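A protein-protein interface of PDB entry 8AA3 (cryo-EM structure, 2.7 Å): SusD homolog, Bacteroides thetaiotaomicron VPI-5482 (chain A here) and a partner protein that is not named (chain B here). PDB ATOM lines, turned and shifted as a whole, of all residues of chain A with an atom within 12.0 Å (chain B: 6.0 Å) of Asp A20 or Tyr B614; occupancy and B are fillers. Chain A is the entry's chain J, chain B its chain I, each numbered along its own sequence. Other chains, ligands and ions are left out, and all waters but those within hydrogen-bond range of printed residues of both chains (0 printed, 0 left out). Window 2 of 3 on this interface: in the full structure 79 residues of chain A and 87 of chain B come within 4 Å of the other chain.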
ATOM      1  N   ASP A  20     -17.461  15.394  -8.758  1.00  0.00           N
ATOM      2  CA  ASP A  20     -17.714  16.820  -8.928  1.00  0.00           C
ATOM      3  C   ASP A  20     -18.952  17.251  -8.147  1.00  0.00           C
ATOM      4  O   ASP A  20     -20.057  17.285  -8.687  1.00  0.00           O
ATOM      5  CB  ASP A  20     -17.878  17.163 -10.412  1.00  0.00           C
ATOM      6  CG  ASP A  20     -17.732  18.647 -10.687  1.00  0.00           C
ATOM      7  OD1 ASP A  20     -17.335  19.389  -9.765  1.00  0.00           O
ATOM      8  OD2 ASP A  20     -18.015  19.071 -11.826  1.00  0.00           O
ATOM      9  N   ASP A  21     -18.754  17.580  -6.872  1.00  0.00           N
ATOM     10  CA  ASP A  21     -19.835  18.008  -5.994  1.00  0.00           C
ATOM     11  C   ASP A  21     -19.929  19.524  -5.876  1.00  0.00           C
ATOM     12  O   ASP A  21     -20.659  20.023  -5.013  1.00  0.00           O
ATOM     13  CB  ASP A  21     -19.664  17.384  -4.607  1.00  0.00           C
ATOM     14  CG  ASP A  21     -18.558  18.042  -3.805  1.00  0.00           C
ATOM     15  OD1 ASP A  21     -17.449  18.218  -4.351  1.00  0.00           O
ATOM     16  OD2 ASP A  21     -18.799  18.384  -2.627  1.00  0.00           O
ATOM     17  N   PHE A  22     -19.202  20.264  -6.716  1.00  0.00           N
ATOM     18  CA  PHE A  22     -19.249  21.722  -6.654  1.00  0.00           C
ATOM     19  C   PHE A  22     -20.640  22.247  -6.986  1.00  0.00           C
ATOM     20  O   PHE A  22     -21.116  23.204  -6.362  1.00  0.00           O
ATOM     21  CB  PHE A  22     -18.209  22.319  -7.601  1.00  0.00           C
ATOM     22  CG  PHE A  22     -18.059  23.807  -7.477  1.00  0.00           C
ATOM     23  CD1 PHE A  22     -17.322  24.358  -6.442  1.00  0.00           C
ATOM     24  CD2 PHE A  22     -18.651  24.657  -8.397  1.00  0.00           C
ATOM     25  CE1 PHE A  22     -17.182  25.727  -6.324  1.00  0.00           C
ATOM     26  CE2 PHE A  22     -18.514  26.028  -8.284  1.00  0.00           C
ATOM     27  CZ  PHE A  22     -17.778  26.563  -7.246  1.00  0.00           C
ATOM     28  N   LEU A  23     -21.306  21.638  -7.964  1.00  0.00           N
ATOM     29  CA  LEU A  23     -22.627  22.072  -8.395  1.00  0.00           C
ATOM     30  C   LEU A  23     -23.757  21.420  -7.608  1.00  0.00           C
ATOM     31  O   LEU A  23     -24.927  21.693  -7.893  1.00  0.00           O
ATOM     32  CB  LEU A  23     -22.808  21.789  -9.890  1.00  0.00           C
ATOM     33  CG  LEU A  23     -21.944  22.628 -10.832  1.00  0.00           C
ATOM     34  CD1 LEU A  23     -22.175  22.234 -12.283  1.00  0.00           C
ATOM     35  CD2 LEU A  23     -22.216  24.110 -10.629  1.00  0.00           C
ATOM     36  N   ASP A  24     -23.440  20.570  -6.630  1.00  0.00           N
ATOM     37  CA  ASP A  24     -24.452  19.907  -5.820  1.00  0.00           C
ATOM     38  C   ASP A  24     -24.324  20.206  -4.332  1.00  0.00           C
ATOM     39  O   ASP A  24     -25.155  19.731  -3.550  1.00  0.00           O
ATOM     40  CB  ASP A  24     -24.398  18.389  -6.040  1.00  0.00           C
ATOM     41  CG  ASP A  24     -25.104  17.959  -7.309  1.00  0.00           C
ATOM     42  OD1 ASP A  24     -26.351  17.881  -7.300  1.00  0.00           O
ATOM     43  OD2 ASP A  24     -24.414  17.698  -8.317  1.00  0.00           O
ATOM     44  N   ARG A  25     -23.309  20.970  -3.919  1.00  0.00           N
ATOM     45  CA  ARG A  25     -23.129  21.261  -2.500  1.00  0.00           C
ATOM     46  C   ARG A  25     -24.280  22.095  -1.948  1.00  0.00           C
ATOM     47  O   ARG A  25     -24.758  21.842  -0.837  1.00  0.00           O
ATOM     48  CB  ARG A  25     -21.797  21.978  -2.278  1.00  0.00           C
ATOM     49  CG  ARG A  25     -21.486  22.273  -0.820  1.00  0.00           C
ATOM     50  CD  ARG A  25     -20.103  22.883  -0.660  1.00  0.00           C
ATOM     51  NE  ARG A  25     -19.045  21.925  -0.957  1.00  0.00           N
ATOM     52  CZ  ARG A  25     -17.756  22.229  -1.021  1.00  0.00           C
ATOM     53  NH1 ARG A  25     -17.325  23.462  -0.812  1.00  0.00           N
ATOM     54  NH2 ARG A  25     -16.877  21.271  -1.301  1.00  0.00           N
ATOM     55  N   GLN A  26     -24.736  23.087  -2.706  1.00  0.00           N
ATOM     56  CA  GLN A  26     -25.771  23.992  -2.227  1.00  0.00           C
ATOM     57  C   GLN A  26     -27.157  23.402  -2.456  1.00  0.00           C
ATOM     58  O   GLN A  26     -27.428  22.792  -3.495  1.00  0.00           O
ATOM     59  CB  GLN A  26     -25.652  25.349  -2.918  1.00  0.00           C
ATOM     60  CG  GLN A  26     -24.383  26.105  -2.556  1.00  0.00           C
ATOM     61  CD  GLN A  26     -24.269  27.433  -3.274  1.00  0.00           C
ATOM     62  OE1 GLN A  26     -25.108  27.772  -4.107  1.00  0.00           O
ATOM     63  NE2 GLN A  26     -23.228  28.191  -2.955  1.00  0.00           N
ATOM     64  N   VAL B 580     -19.875  26.404 -13.474  1.00  0.00           N
ATOM     65  CA  VAL B 580     -18.645  25.757 -13.915  1.00  0.00           C
ATOM     66  C   VAL B 580     -18.521  25.964 -15.419  1.00  0.00           C
ATOM     67  O   VAL B 580     -19.487  25.745 -16.159  1.00  0.00           O
ATOM     68  CB  VAL B 580     -18.629  24.256 -13.569  1.00  0.00           C
ATOM     69  CG1 VAL B 580     -17.369  23.596 -14.108  1.00  0.00           C
ATOM     70  CG2 VAL B 580     -18.739  24.054 -12.066  1.00  0.00           C
ATOM     71  N   PHE B 582     -15.794  25.539 -18.927  1.00  0.00           N
ATOM     72  CA  PHE B 582     -14.573  25.133 -19.616  1.00  0.00           C
ATOM     73  C   PHE B 582     -14.613  25.745 -21.010  1.00  0.00           C
ATOM     74  O   PHE B 582     -15.473  25.391 -21.821  1.00  0.00           O
ATOM     75  CB  PHE B 582     -14.451  23.611 -19.691  1.00  0.00           C
ATOM     76  CG  PHE B 582     -14.607  22.922 -18.367  1.00  0.00           C
ATOM     77  CD1 PHE B 582     -13.542  22.837 -17.484  1.00  0.00           C
ATOM     78  CD2 PHE B 582     -15.815  22.348 -18.007  1.00  0.00           C
ATOM     79  CE1 PHE B 582     -13.682  22.198 -16.266  1.00  0.00           C
ATOM     80  CE2 PHE B 582     -15.961  21.709 -16.792  1.00  0.00           C
ATOM     81  CZ  PHE B 582     -14.893  21.634 -15.919  1.00  0.00           C
ATOM     82  N   ARG B 602     -18.210  24.997 -22.620  1.00  0.00           N
ATOM     83  CA  ARG B 602     -18.985  23.972 -21.929  1.00  0.00           C
ATOM     84  C   ARG B 602     -19.354  24.543 -20.568  1.00  0.00           C
ATOM     85  O   ARG B 602     -18.483  24.720 -19.707  1.00  0.00           O
ATOM     86  CB  ARG B 602     -18.191  22.673 -21.792  1.00  0.00           C
ATOM     87  CG  ARG B 602     -18.979  21.519 -21.193  1.00  0.00           C
ATOM     88  CD  ARG B 602     -19.927  20.909 -22.213  1.00  0.00           C
ATOM     89  NE  ARG B 602     -20.537  19.678 -21.722  1.00  0.00           N
ATOM     90  CZ  ARG B 602     -21.661  19.160 -22.196  1.00  0.00           C
ATOM     91  NH1 ARG B 602     -22.329  19.739 -23.180  1.00  0.00           N
ATOM     92  NH2 ARG B 602     -22.126  18.030 -21.670  1.00  0.00           N
ATOM     93  N   ASP B 603     -20.636  24.847 -20.379  1.00  0.00           N
ATOM     94  CA  ASP B 603     -21.103  25.574 -19.207  1.00  0.00           C
ATOM     95  C   ASP B 603     -22.138  24.756 -18.450  1.00  0.00           C
ATOM     96  O   ASP B 603     -23.036  24.159 -19.052  1.00  0.00           O
ATOM     97  CB  ASP B 603     -21.702  26.926 -19.608  1.00  0.00           C
ATOM     98  CG  ASP B 603     -20.679  27.855 -20.233  1.00  0.00           C
ATOM     99  OD1 ASP B 603     -19.483  27.736 -19.894  1.00  0.00           O
ATOM    100  OD2 ASP B 603     -21.071  28.701 -21.064  1.00  0.00           O
ATOM    101  N   GLY B 604     -22.009  24.742 -17.130  1.00  0.00           N
ATOM    102  CA  GLY B 604     -22.961  24.054 -16.279  1.00  0.00           C
ATOM    103  C   GLY B 604     -23.291  24.893 -15.064  1.00  0.00           C
ATOM    104  O   GLY B 604     -22.463  25.661 -14.569  1.00  0.00           O
ATOM    105  N   SER B 605     -24.522  24.737 -14.585  1.00  0.00           N
ATOM    106  CA  SER B 605     -25.011  25.504 -13.449  1.00  0.00           C
ATOM    107  C   SER B 605     -25.748  24.581 -12.491  1.00  0.00           C
ATOM    108  O   SER B 605     -26.249  23.521 -12.874  1.00  0.00           O
ATOM    109  CB  SER B 605     -25.932  26.647 -13.892  1.00  0.00           C
ATOM    110  OG  SER B 605     -27.149  26.148 -14.416  1.00  0.00           O
ATOM    111  N   GLY B 609     -31.021  20.307 -13.446  1.00  0.00           N
ATOM    112  CA  GLY B 609     -30.804  18.939 -13.032  1.00  0.00           C
ATOM    113  C   GLY B 609     -29.520  18.368 -13.605  1.00  0.00           C
ATOM    114  O   GLY B 609     -28.850  18.965 -14.448  1.00  0.00           O
ATOM    115  N   LYS B 610     -29.173  17.172 -13.123  1.00  0.00           N
ATOM    116  CA  LYS B 610     -27.938  16.530 -13.559  1.00  0.00           C
ATOM    117  C   LYS B 610     -27.980  16.187 -15.044  1.00  0.00           C
ATOM    118  O   LYS B 610     -26.963  16.284 -15.741  1.00  0.00           O
ATOM    119  CB  LYS B 610     -27.676  15.275 -12.727  1.00  0.00           C
ATOM    120  CG  LYS B 610     -27.269  15.558 -11.290  1.00  0.00           C
ATOM    121  CD  LYS B 610     -26.986  14.270 -10.534  1.00  0.00           C
ATOM    122  CE  LYS B 610     -26.594  14.551  -9.092  1.00  0.00           C
ATOM    123  NZ  LYS B 610     -25.264  15.215  -8.999  1.00  0.00           N
ATOM    124  N   ASN B 611     -29.148  15.773 -15.543  1.00  0.00           N
ATOM    125  CA  ASN B 611     -29.257  15.378 -16.945  1.00  0.00           C
ATOM    126  C   ASN B 611     -29.003  16.555 -17.881  1.00  0.00           C
ATOM    127  O   ASN B 611     -28.325  16.407 -18.905  1.00  0.00           O
ATOM    128  CB  ASN B 611     -30.635  14.771 -17.211  1.00  0.00           C
ATOM    129  CG  ASN B 611     -30.906  13.547 -16.358  1.00  0.00           C
ATOM    130  OD1 ASN B 611     -30.082  12.636 -16.280  1.00  0.00           O
ATOM    131  ND2 ASN B 611     -32.066  13.521 -15.712  1.00  0.00           N
ATOM    132  N   HIS B 612     -29.536  17.731 -17.548  1.00  0.00           N
ATOM    133  CA  HIS B 612     -29.408  18.919 -18.384  1.00  0.00           C
ATOM    134  C   HIS B 612     -28.518  19.978 -17.741  1.00  0.00           C
ATOM    135  O   HIS B 612     -28.742  21.178 -17.918  1.00  0.00           O
ATOM    136  CB  HIS B 612     -30.787  19.503 -18.692  1.00  0.00           C
ATOM    137  CG  HIS B 612     -31.678  18.575 -19.458  1.00  0.00           C
ATOM    138  ND1 HIS B 612     -31.516  18.329 -20.804  1.00  0.00           N
ATOM    139  CD2 HIS B 612     -32.741  17.835 -19.066  1.00  0.00           C
ATOM    140  CE1 HIS B 612     -32.441  17.477 -21.209  1.00  0.00           C
ATOM    141  NE2 HIS B 612     -33.198  17.161 -20.173  1.00  0.00           N
ATOM    142  N   ARG B 613     -27.504  19.547 -16.988  1.00  0.00           N
ATOM    143  CA  ARG B 613     -26.653  20.495 -16.277  1.00  0.00           C
ATOM    144  C   ARG B 613     -25.728  21.242 -17.230  1.00  0.00           C
ATOM    145  O   ARG B 613     -25.583  22.466 -17.138  1.00  0.00           O
ATOM    146  CB  ARG B 613     -25.845  19.767 -15.203  1.00  0.00           C
ATOM    147  CG  ARG B 613     -25.133  20.688 -14.228  1.00  0.00           C
ATOM    148  CD  ARG B 613     -25.036  20.057 -12.850  1.00  0.00           C
ATOM    149  NE  ARG B 613     -26.312  20.089 -12.146  1.00  0.00           N
ATOM    150  CZ  ARG B 613     -26.484  19.705 -10.888  1.00  0.00           C
ATOM    151  NH1 ARG B 613     -25.477  19.248 -10.162  1.00  0.00           N
ATOM    152  NH2 ARG B 613     -27.695  19.781 -10.346  1.00  0.00           N
ATOM    153  N   TYR B 614     -25.103  20.527 -18.161  1.00  0.00           N
ATOM    154  CA  TYR B 614     -24.065  21.088 -19.010  1.00  0.00           C
ATOM    155  C   TYR B 614     -24.574  21.301 -20.430  1.00  0.00           C
ATOM    156  O   TYR B 614     -25.401  20.538 -20.938  1.00  0.00           O
ATOM    157  CB  TYR B 614     -22.828  20.183 -19.034  1.00  0.00           C
ATOM    158  CG  TYR B 614     -22.026  20.215 -17.752  1.00  0.00           C
ATOM    159  CD1 TYR B 614     -22.337  19.373 -16.694  1.00  0.00           C
ATOM    160  CD2 TYR B 614     -20.958  21.091 -17.602  1.00  0.00           C
ATOM    161  CE1 TYR B 614     -21.606  19.400 -15.520  1.00  0.00           C
ATOM    162  CE2 TYR B 614     -20.222  21.126 -16.433  1.00  0.00           C
ATOM    163  CZ  TYR B 614     -20.550  20.278 -15.395  1.00  0.00           C
ATOM    164  OH  TYR B 614     -19.820  20.309 -14.230  1.00  0.00           O
ATOM    165  N   ALA B 615     -24.066  22.356 -21.064  1.00  0.00           N
ATOM    166  CA  ALA B 615     -24.422  22.699 -22.433  1.00  0.00           C
ATOM    167  C   ALA B 615     -23.190  23.223 -23.159  1.00  0.00           C
ATOM    168  O   ALA B 615     -22.250  23.734 -22.544  1.00  0.00           O
ATOM    169  CB  ALA B 615     -25.553  23.733 -22.481  1.00  0.00           C
ATOM    170  N   THR B 616     -23.212  23.095 -24.484  1.00  0.00           N
ATOM    171  CA  THR B 616     -22.089  23.454 -25.340  1.00  0.00           C
ATOM    172  C   THR B 616     -22.485  24.594 -26.269  1.00  0.00           C
ATOM    173  O   THR B 616     -23.571  24.583 -26.856  1.00  0.00           O
ATOM    174  CB  THR B 616     -21.616  22.247 -26.163  1.00  0.00           C
ATOM    175  OG1 THR B 616     -21.242  21.182 -25.281  1.00  0.00           O
ATOM    176  CG2 THR B 616     -20.419  22.619 -27.026  1.00  0.00           C
ATOM    177  N   TRP B 710     -30.556  25.217 -20.677  1.00  0.00           N
ATOM    178  CA  TRP B 710     -30.040  26.539 -21.001  1.00  0.00           C
ATOM    179  C   TRP B 710     -30.827  27.166 -22.147  1.00  0.00           C
ATOM    180  O   TRP B 710     -31.306  26.478 -23.053  1.00  0.00           O
ATOM    181  CB  TRP B 710     -28.561  26.453 -21.380  1.00  0.00           C
ATOM    182  CG  TRP B 710     -27.655  26.130 -20.232  1.00  0.00           C
ATOM    183  CD1 TRP B 710     -27.574  24.944 -19.560  1.00  0.00           C
ATOM    184  CD2 TRP B 710     -26.685  26.997 -19.633  1.00  0.00           C
ATOM    185  NE1 TRP B 710     -26.622  25.024 -18.572  1.00  0.00           N
ATOM    186  CE2 TRP B 710     -26.061  26.274 -18.597  1.00  0.00           C
ATOM    187  CE3 TRP B 710     -26.287  28.317 -19.869  1.00  0.00           C
ATOM    188  CZ2 TRP B 710     -25.060  26.825 -17.799  1.00  0.00           C
ATOM    189  CZ3 TRP B 710     -25.294  28.862 -19.075  1.00  0.00           C
ATOM    190  CH2 TRP B 710     -24.693  28.118 -18.053  1.00  0.00           C
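OD2 of Asp A20 lies within hydrogen-bond range of OH of Tyr B614 (3.3 Å).
The side-chain amino group (NZ) of Lys B610 lies within salt-bridge range of the side-chain carboxylate (OD2) of Asp A24 (2.7 Å).
NH1 of Arg B613 sits at hydrogen-bond distance from O of Leu A23, at 3.4 Å.
The guanidinium group (NH1) of Arg B613 is in salt-bridge range of the side-chain carboxylate (OD2) of Asp A24.
The backbone carbonyl oxygen of Val B580 is in hydrogen-bond range of the backbone NH of Gly B604 (2.9 Å).
O of Arg B613 sits at hydrogen-bond distance from NE1 of Trp B710 (3.1 Å).
Among the printed residues, merely in contact across the chains: Phe A22 with Val B580 (3.7 Å), Leu A23 with Val B580 (3.7 Å) and Leu A23 with Tyr B614 (3.6 Å).
Of chain B, only Tyr B614 (3.3 Å) comes within 4 Å of Asp A20.
Of chain A, only Asp A20 (3.3 Å) and Leu A23 (3.6 Å) come within 4 Å of Tyr B614.
Val B580 touches two residues of chain A.
No residue of chain A comes within 4 Å of Arg B602.
No residue of chain A comes within 4 Å of Gly B609.
Lys B610 touches just one residue of chain A: Asp A24.
Of the printed residues of chain B, Asp A24 touches Lys B610 (2.7 Å) and Arg B613 (2.6 Å).
Of the printed residues of chain A, Arg B613 touches Leu A23 and Asp A24.
Of the printed residues of chain B, Phe A22 touches Val B580 (3.7 Å).
Gly B604 touches none of the printed residues of chain A.
His B612 touches none of the printed residues of chain A.
The nearest residue of chain B that does not touch Asp A20 is Val B580 (5.0 Å).
The nearest residue of chain A that does not touch Tyr B614 is Phe A22 (7.1 Å).
Hydrophobic or aromatic side chains of chain B that line the printed part of chain A: Val B580 and Tyr B614.
Of the 7 printed residues of chain A, 4 touch a printed residue of chain B.
Among the printed residues, Asp or Glu carboxylates within 4 Å of a Lys or Arg side-chain nitrogen of the other chain: Asp A24 with Lys B610 and Asp A24 with Arg B613.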
